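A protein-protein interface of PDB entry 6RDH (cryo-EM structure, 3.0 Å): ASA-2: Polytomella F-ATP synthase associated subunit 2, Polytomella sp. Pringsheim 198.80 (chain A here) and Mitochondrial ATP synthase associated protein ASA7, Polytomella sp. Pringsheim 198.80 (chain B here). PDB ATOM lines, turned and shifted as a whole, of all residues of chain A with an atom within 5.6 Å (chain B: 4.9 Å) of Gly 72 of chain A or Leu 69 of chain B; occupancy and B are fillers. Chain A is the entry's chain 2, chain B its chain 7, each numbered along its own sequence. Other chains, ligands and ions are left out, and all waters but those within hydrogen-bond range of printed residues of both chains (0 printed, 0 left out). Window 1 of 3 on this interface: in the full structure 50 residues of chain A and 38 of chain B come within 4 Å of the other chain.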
ATOM      1  N   THR A  33       5.506  10.685  15.149  1.00  0.00           N
ATOM      2  CA  THR A  33       5.616  10.260  13.750  1.00  0.00           C
ATOM      3  C   THR A  33       7.055  10.056  13.330  1.00  0.00           C
ATOM      4  O   THR A  33       7.359   9.091  12.623  1.00  0.00           O
ATOM      5  CB  THR A  33       5.002  11.269  12.793  1.00  0.00           C
ATOM      6  OG1 THR A  33       5.763  12.479  12.810  1.00  0.00           O
ATOM      7  CG2 THR A  33       3.640  11.549  13.187  1.00  0.00           C
ATOM      8  N   GLN A  36       8.149   6.861  14.137  1.00  0.00           N
ATOM      9  CA  GLN A  36       7.388   5.863  13.372  1.00  0.00           C
ATOM     10  C   GLN A  36       6.793   4.778  14.278  1.00  0.00           C
ATOM     11  O   GLN A  36       7.182   3.609  14.241  1.00  0.00           O
ATOM     12  CB  GLN A  36       8.256   5.250  12.270  1.00  0.00           C
ATOM     13  CG  GLN A  36       8.772   6.253  11.265  1.00  0.00           C
ATOM     14  CD  GLN A  36       9.649   5.608  10.225  1.00  0.00           C
ATOM     15  OE1 GLN A  36       9.254   4.641   9.577  1.00  0.00           O
ATOM     16  NE2 GLN A  36      10.857   6.128  10.069  1.00  0.00           N
ATOM     17  N   VAL A  37       5.820   5.200  15.086  1.00  0.00           N
ATOM     18  CA  VAL A  37       5.379   4.426  16.243  1.00  0.00           C
ATOM     19  C   VAL A  37       3.958   3.927  15.973  1.00  0.00           C
ATOM     20  O   VAL A  37       3.038   4.109  16.776  1.00  0.00           O
ATOM     21  CB  VAL A  37       5.501   5.236  17.551  1.00  0.00           C
ATOM     22  CG1 VAL A  37       5.450   4.325  18.779  1.00  0.00           C
ATOM     23  CG2 VAL A  37       6.798   5.992  17.576  1.00  0.00           C
ATOM     24  N   LYS A  38       3.739   3.395  14.772  1.00  0.00           N
ATOM     25  CA  LYS A  38       2.515   2.655  14.475  1.00  0.00           C
ATOM     26  C   LYS A  38       2.310   1.414  15.342  1.00  0.00           C
ATOM     27  O   LYS A  38       1.193   0.890  15.376  1.00  0.00           O
ATOM     28  CB  LYS A  38       2.510   2.235  13.011  1.00  0.00           C
ATOM     29  CG  LYS A  38       2.467   3.395  12.054  1.00  0.00           C
ATOM     30  CD  LYS A  38       1.051   3.745  11.710  1.00  0.00           C
ATOM     31  CE  LYS A  38       0.416   2.599  10.969  1.00  0.00           C
ATOM     32  NZ  LYS A  38       1.149   2.302   9.711  1.00  0.00           N
ATOM     33  N   TRP A  44      -0.835   6.978  20.620  1.00  0.00           N
ATOM     34  CA  TRP A  44      -1.524   7.848  19.682  1.00  0.00           C
ATOM     35  C   TRP A  44      -2.917   8.191  20.172  1.00  0.00           C
ATOM     36  O   TRP A  44      -3.404   9.299  19.924  1.00  0.00           O
ATOM     37  CB  TRP A  44      -1.587   7.191  18.315  1.00  0.00           C
ATOM     38  CG  TRP A  44      -0.443   7.543  17.460  1.00  0.00           C
ATOM     39  CD1 TRP A  44       0.577   6.730  17.089  1.00  0.00           C
ATOM     40  CD2 TRP A  44      -0.183   8.812  16.865  1.00  0.00           C
ATOM     41  NE1 TRP A  44       1.454   7.410  16.296  1.00  0.00           N
ATOM     42  CE2 TRP A  44       1.008   8.693  16.143  1.00  0.00           C
ATOM     43  CE3 TRP A  44      -0.849  10.039  16.872  1.00  0.00           C
ATOM     44  CZ2 TRP A  44       1.549   9.748  15.434  1.00  0.00           C
ATOM     45  CZ3 TRP A  44      -0.309  11.086  16.167  1.00  0.00           C
ATOM     46  CH2 TRP A  44       0.877  10.934  15.458  1.00  0.00           C
ATOM     47  N   TRP A  67      -0.277  17.906  10.436  1.00  0.00           N
ATOM     48  CA  TRP A  67       0.768  17.255   9.654  1.00  0.00           C
ATOM     49  C   TRP A  67       1.153  15.915  10.256  1.00  0.00           C
ATOM     50  O   TRP A  67       1.349  14.939   9.528  1.00  0.00           O
ATOM     51  CB  TRP A  67       2.006  18.151   9.555  1.00  0.00           C
ATOM     52  CG  TRP A  67       3.150  17.472   8.850  1.00  0.00           C
ATOM     53  CD1 TRP A  67       3.391  17.475   7.517  1.00  0.00           C
ATOM     54  CD2 TRP A  67       4.190  16.684   9.444  1.00  0.00           C
ATOM     55  NE1 TRP A  67       4.508  16.735   7.237  1.00  0.00           N
ATOM     56  CE2 TRP A  67       5.012  16.235   8.406  1.00  0.00           C
ATOM     57  CE3 TRP A  67       4.493  16.304  10.752  1.00  0.00           C
ATOM     58  CZ2 TRP A  67       6.121  15.436   8.631  1.00  0.00           C
ATOM     59  CZ3 TRP A  67       5.592  15.509  10.971  1.00  0.00           C
ATOM     60  CH2 TRP A  67       6.394  15.084   9.922  1.00  0.00           C
ATOM     61  N   ALA A  68       1.271  15.850  11.581  1.00  0.00           N
ATOM     62  CA  ALA A  68       1.653  14.605  12.229  1.00  0.00           C
ATOM     63  C   ALA A  68       0.550  13.567  12.151  1.00  0.00           C
ATOM     64  O   ALA A  68       0.836  12.379  11.983  1.00  0.00           O
ATOM     65  CB  ALA A  68       2.024  14.878  13.677  1.00  0.00           C
ATOM     66  N   ILE A  69      -0.707  13.997  12.249  1.00  0.00           N
ATOM     67  CA  ILE A  69      -1.830  13.069  12.150  1.00  0.00           C
ATOM     68  C   ILE A  69      -1.857  12.417  10.775  1.00  0.00           C
ATOM     69  O   ILE A  69      -2.030  11.200  10.650  1.00  0.00           O
ATOM     70  CB  ILE A  69      -3.146  13.803  12.469  1.00  0.00           C
ATOM     71  CG1 ILE A  69      -3.265  14.028  13.971  1.00  0.00           C
ATOM     72  CG2 ILE A  69      -4.351  13.023  11.991  1.00  0.00           C
ATOM     73  CD1 ILE A  69      -4.348  14.982  14.345  1.00  0.00           C
ATOM     74  N   ASN A  70      -1.587  13.197   9.731  1.00  0.00           N
ATOM     75  CA  ASN A  70      -1.662  12.630   8.386  1.00  0.00           C
ATOM     76  C   ASN A  70      -0.378  11.958   7.929  1.00  0.00           C
ATOM     77  O   ASN A  70      -0.426  11.091   7.054  1.00  0.00           O
ATOM     78  CB  ASN A  70      -2.086  13.719   7.430  1.00  0.00           C
ATOM     79  CG  ASN A  70      -3.556  13.851   7.401  1.00  0.00           C
ATOM     80  OD1 ASN A  70      -4.097  14.789   7.939  1.00  0.00           O
ATOM     81  ND2 ASN A  70      -4.223  12.935   6.724  1.00  0.00           N
ATOM     82  N   THR A  71       0.768  12.316   8.500  1.00  0.00           N
ATOM     83  CA  THR A  71       1.988  11.593   8.174  1.00  0.00           C
ATOM     84  C   THR A  71       2.032  10.255   8.891  1.00  0.00           C
ATOM     85  O   THR A  71       2.466   9.251   8.316  1.00  0.00           O
ATOM     86  CB  THR A  71       3.202  12.440   8.530  1.00  0.00           C
ATOM     87  OG1 THR A  71       3.047  13.740   7.954  1.00  0.00           O
ATOM     88  CG2 THR A  71       4.465  11.815   7.996  1.00  0.00           C
ATOM     89  N   GLY A  72       1.565  10.212  10.139  1.00  0.00           N
ATOM     90  CA  GLY A  72       1.525   8.955  10.856  1.00  0.00           C
ATOM     91  C   GLY A  72       0.448   8.015  10.374  1.00  0.00           C
ATOM     92  O   GLY A  72       0.505   6.820  10.671  1.00  0.00           O
ATOM     93  N   GLY A  73      -0.527   8.526   9.633  1.00  0.00           N
ATOM     94  CA  GLY A  73      -1.593   7.686   9.131  1.00  0.00           C
ATOM     95  C   GLY A  73      -2.594   7.266  10.177  1.00  0.00           C
ATOM     96  O   GLY A  73      -3.216   6.213  10.038  1.00  0.00           O
ATOM     97  N   VAL A  74      -2.759   8.046  11.224  1.00  0.00           N
ATOM     98  CA  VAL A  74      -3.752   7.741  12.242  1.00  0.00           C
ATOM     99  C   VAL A  74      -5.079   8.341  11.812  1.00  0.00           C
ATOM    100  O   VAL A  74      -5.138   9.360  11.116  1.00  0.00           O
ATOM    101  CB  VAL A  74      -3.307   8.236  13.635  1.00  0.00           C
ATOM    102  CG1 VAL A  74      -1.911   7.766  13.911  1.00  0.00           C
ATOM    103  CG2 VAL A  74      -3.360   9.739  13.745  1.00  0.00           C
ATOM    104  N   ALA B  65      10.133   6.571   4.154  1.00  0.00           N
ATOM    105  CA  ALA B  65       9.577   6.059   5.399  1.00  0.00           C
ATOM    106  C   ALA B  65       8.391   6.875   5.884  1.00  0.00           C
ATOM    107  O   ALA B  65       7.407   6.304   6.358  1.00  0.00           O
ATOM    108  CB  ALA B  65      10.649   6.023   6.486  1.00  0.00           C
ATOM    109  N   LEU B  66       8.459   8.200   5.770  1.00  0.00           N
ATOM    110  CA  LEU B  66       7.312   9.027   6.114  1.00  0.00           C
ATOM    111  C   LEU B  66       6.197   8.933   5.080  1.00  0.00           C
ATOM    112  O   LEU B  66       5.049   9.271   5.390  1.00  0.00           O
ATOM    113  CB  LEU B  66       7.740  10.483   6.288  1.00  0.00           C
ATOM    114  CG  LEU B  66       8.571  10.811   7.527  1.00  0.00           C
ATOM    115  CD1 LEU B  66       8.406  12.278   7.851  1.00  0.00           C
ATOM    116  CD2 LEU B  66       8.194   9.958   8.729  1.00  0.00           C
ATOM    117  N   ARG B  67       6.502   8.500   3.860  1.00  0.00           N
ATOM    118  CA  ARG B  67       5.451   8.181   2.910  1.00  0.00           C
ATOM    119  C   ARG B  67       4.949   6.758   3.078  1.00  0.00           C
ATOM    120  O   ARG B  67       3.816   6.463   2.692  1.00  0.00           O
ATOM    121  CB  ARG B  67       5.955   8.393   1.486  1.00  0.00           C
ATOM    122  CG  ARG B  67       6.320   9.825   1.176  1.00  0.00           C
ATOM    123  CD  ARG B  67       5.082  10.680   1.094  1.00  0.00           C
ATOM    124  NE  ARG B  67       4.032  10.022   0.326  1.00  0.00           N
ATOM    125  CZ  ARG B  67       3.917  10.094  -0.995  1.00  0.00           C
ATOM    126  NH1 ARG B  67       4.788  10.802  -1.699  1.00  0.00           N
ATOM    127  NH2 ARG B  67       2.930   9.461  -1.612  1.00  0.00           N
ATOM    128  N   LYS B  68       5.768   5.874   3.639  1.00  0.00           N
ATOM    129  CA  LYS B  68       5.351   4.502   3.871  1.00  0.00           C
ATOM    130  C   LYS B  68       4.619   4.337   5.193  1.00  0.00           C
ATOM    131  O   LYS B  68       4.134   3.239   5.484  1.00  0.00           O
ATOM    132  CB  LYS B  68       6.563   3.573   3.841  1.00  0.00           C
ATOM    133  CG  LYS B  68       6.287   2.217   3.230  1.00  0.00           C
ATOM    134  CD  LYS B  68       7.323   1.190   3.646  1.00  0.00           C
ATOM    135  CE  LYS B  68       8.718   1.600   3.219  1.00  0.00           C
ATOM    136  NZ  LYS B  68       8.859   1.666   1.743  1.00  0.00           N
ATOM    137  N   LEU B  69       4.532   5.400   5.996  1.00  0.00           N
ATOM    138  CA  LEU B  69       3.935   5.280   7.322  1.00  0.00           C
ATOM    139  C   LEU B  69       2.418   5.199   7.243  1.00  0.00           C
ATOM    140  O   LEU B  69       1.796   4.432   7.985  1.00  0.00           O
ATOM    141  CB  LEU B  69       4.371   6.452   8.197  1.00  0.00           C
ATOM    142  CG  LEU B  69       4.383   6.212   9.704  1.00  0.00           C
ATOM    143  CD1 LEU B  69       5.192   4.987  10.044  1.00  0.00           C
ATOM    144  CD2 LEU B  69       4.946   7.423  10.403  1.00  0.00           C
ATOM    145  N   SER B  70       1.804   5.956   6.336  1.00  0.00           N
ATOM    146  CA  SER B  70       0.357   5.941   6.176  1.00  0.00           C
ATOM    147  C   SER B  70      -0.120   4.851   5.225  1.00  0.00           C
ATOM    148  O   SER B  70      -1.208   4.972   4.660  1.00  0.00           O
ATOM    149  CB  SER B  70      -0.138   7.302   5.691  1.00  0.00           C
ATOM    150  OG  SER B  70       0.189   7.512   4.335  1.00  0.00           O
ATOM    151  N   GLY B  71       0.672   3.803   5.021  1.00  0.00           N
ATOM    152  CA  GLY B  71       0.255   2.681   4.206  1.00  0.00           C
ATOM    153  C   GLY B  71      -0.730   1.821   4.961  1.00  0.00           C
ATOM    154  O   GLY B  71      -1.738   1.371   4.412  1.00  0.00           O
ATOM    155  N   SER B  72      -0.436   1.578   6.227  1.00  0.00           N
ATOM    156  CA  SER B  72      -1.417   1.029   7.146  1.00  0.00           C
ATOM    157  C   SER B  72      -1.951   2.160   8.009  1.00  0.00           C
ATOM    158  O   SER B  72      -1.269   3.159   8.243  1.00  0.00           O
ATOM    159  CB  SER B  72      -0.815  -0.064   8.024  1.00  0.00           C
ATOM    160  OG  SER B  72      -1.635  -0.296   9.155  1.00  0.00           O
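Printed residues of chain B within 4 Å of Trp 67 of chain A: Leu 66 (3.98 Å).
Of the printed residues of chain B, Thr 71 of chain A touches Leu 66 (3.7 Å), Leu 69 (3.4 Å) and Ser 70 (3.9 Å).
Of chain B, only Leu 69 comes within 4 Å of Gly 72 of chain A.
Of the printed residues of chain A, Ala 65 of chain B touches Gln 36.
Lys 68 of chain B touches none of the printed residues of chain A.
Leu 69 of chain B touches five residues of chain A.
Of the printed residues of chain A, Ser 70 of chain B touches Thr 71 (3.9 Å) and Gly 73 (3.8 Å).
Printed residues of chain A within 4 Å of Ser 72 of chain B: Lys 38 (3.0 Å).
The nearest residue of chain B that does not touch Gly 72 of chain A is Ser 70 of chain B (4.6 Å).
O of Trp 67 of chain A sits at hydrogen-bond distance from OG1 of Thr 71 of chain A (2.6 Å).
Hydrophobic or aromatic side chains of chain B that line the printed part of chain A: Ala 65, Leu 66 and Leu 69.
Along chain B the printed residues that touch a printed residue of chain A span positions 65 to 72.
Among the printed residues, no Asp or Glu carboxylate lies within 4 Å of a Lys or Arg side-chain nitrogen of the other chain.
Among the printed residues, pairs that only touch across the chains: Thr 33 of chain A with Leu 69 of chain B, Gln 36 of chain A with Ala 65 of chain B, Gln 36 of chain A with Leu 69 of chain B, Trp 67 of chain A with Leu 66 of chain B, Thr 71 of chain A with Leu 66 of chain B, Thr 71 of chain A with Leu 69 of chain B, Thr 71 of chain A with Ser 70 of chain B, Gly 72 of chain A with Leu 69 of chain B and Gly 73 of chain A with Ser 70 of chain B.
NZ of Lys 38 of chain A sits at hydrogen-bond distance from O of Leu 69 of chain B (2.8 Å).
The side-chain amino group (NZ) of Lys 38 of chain A sits at hydrogen-bond distance from the backbone carbonyl oxygen (O) of Ser 72 of chain B (3.0 Å).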
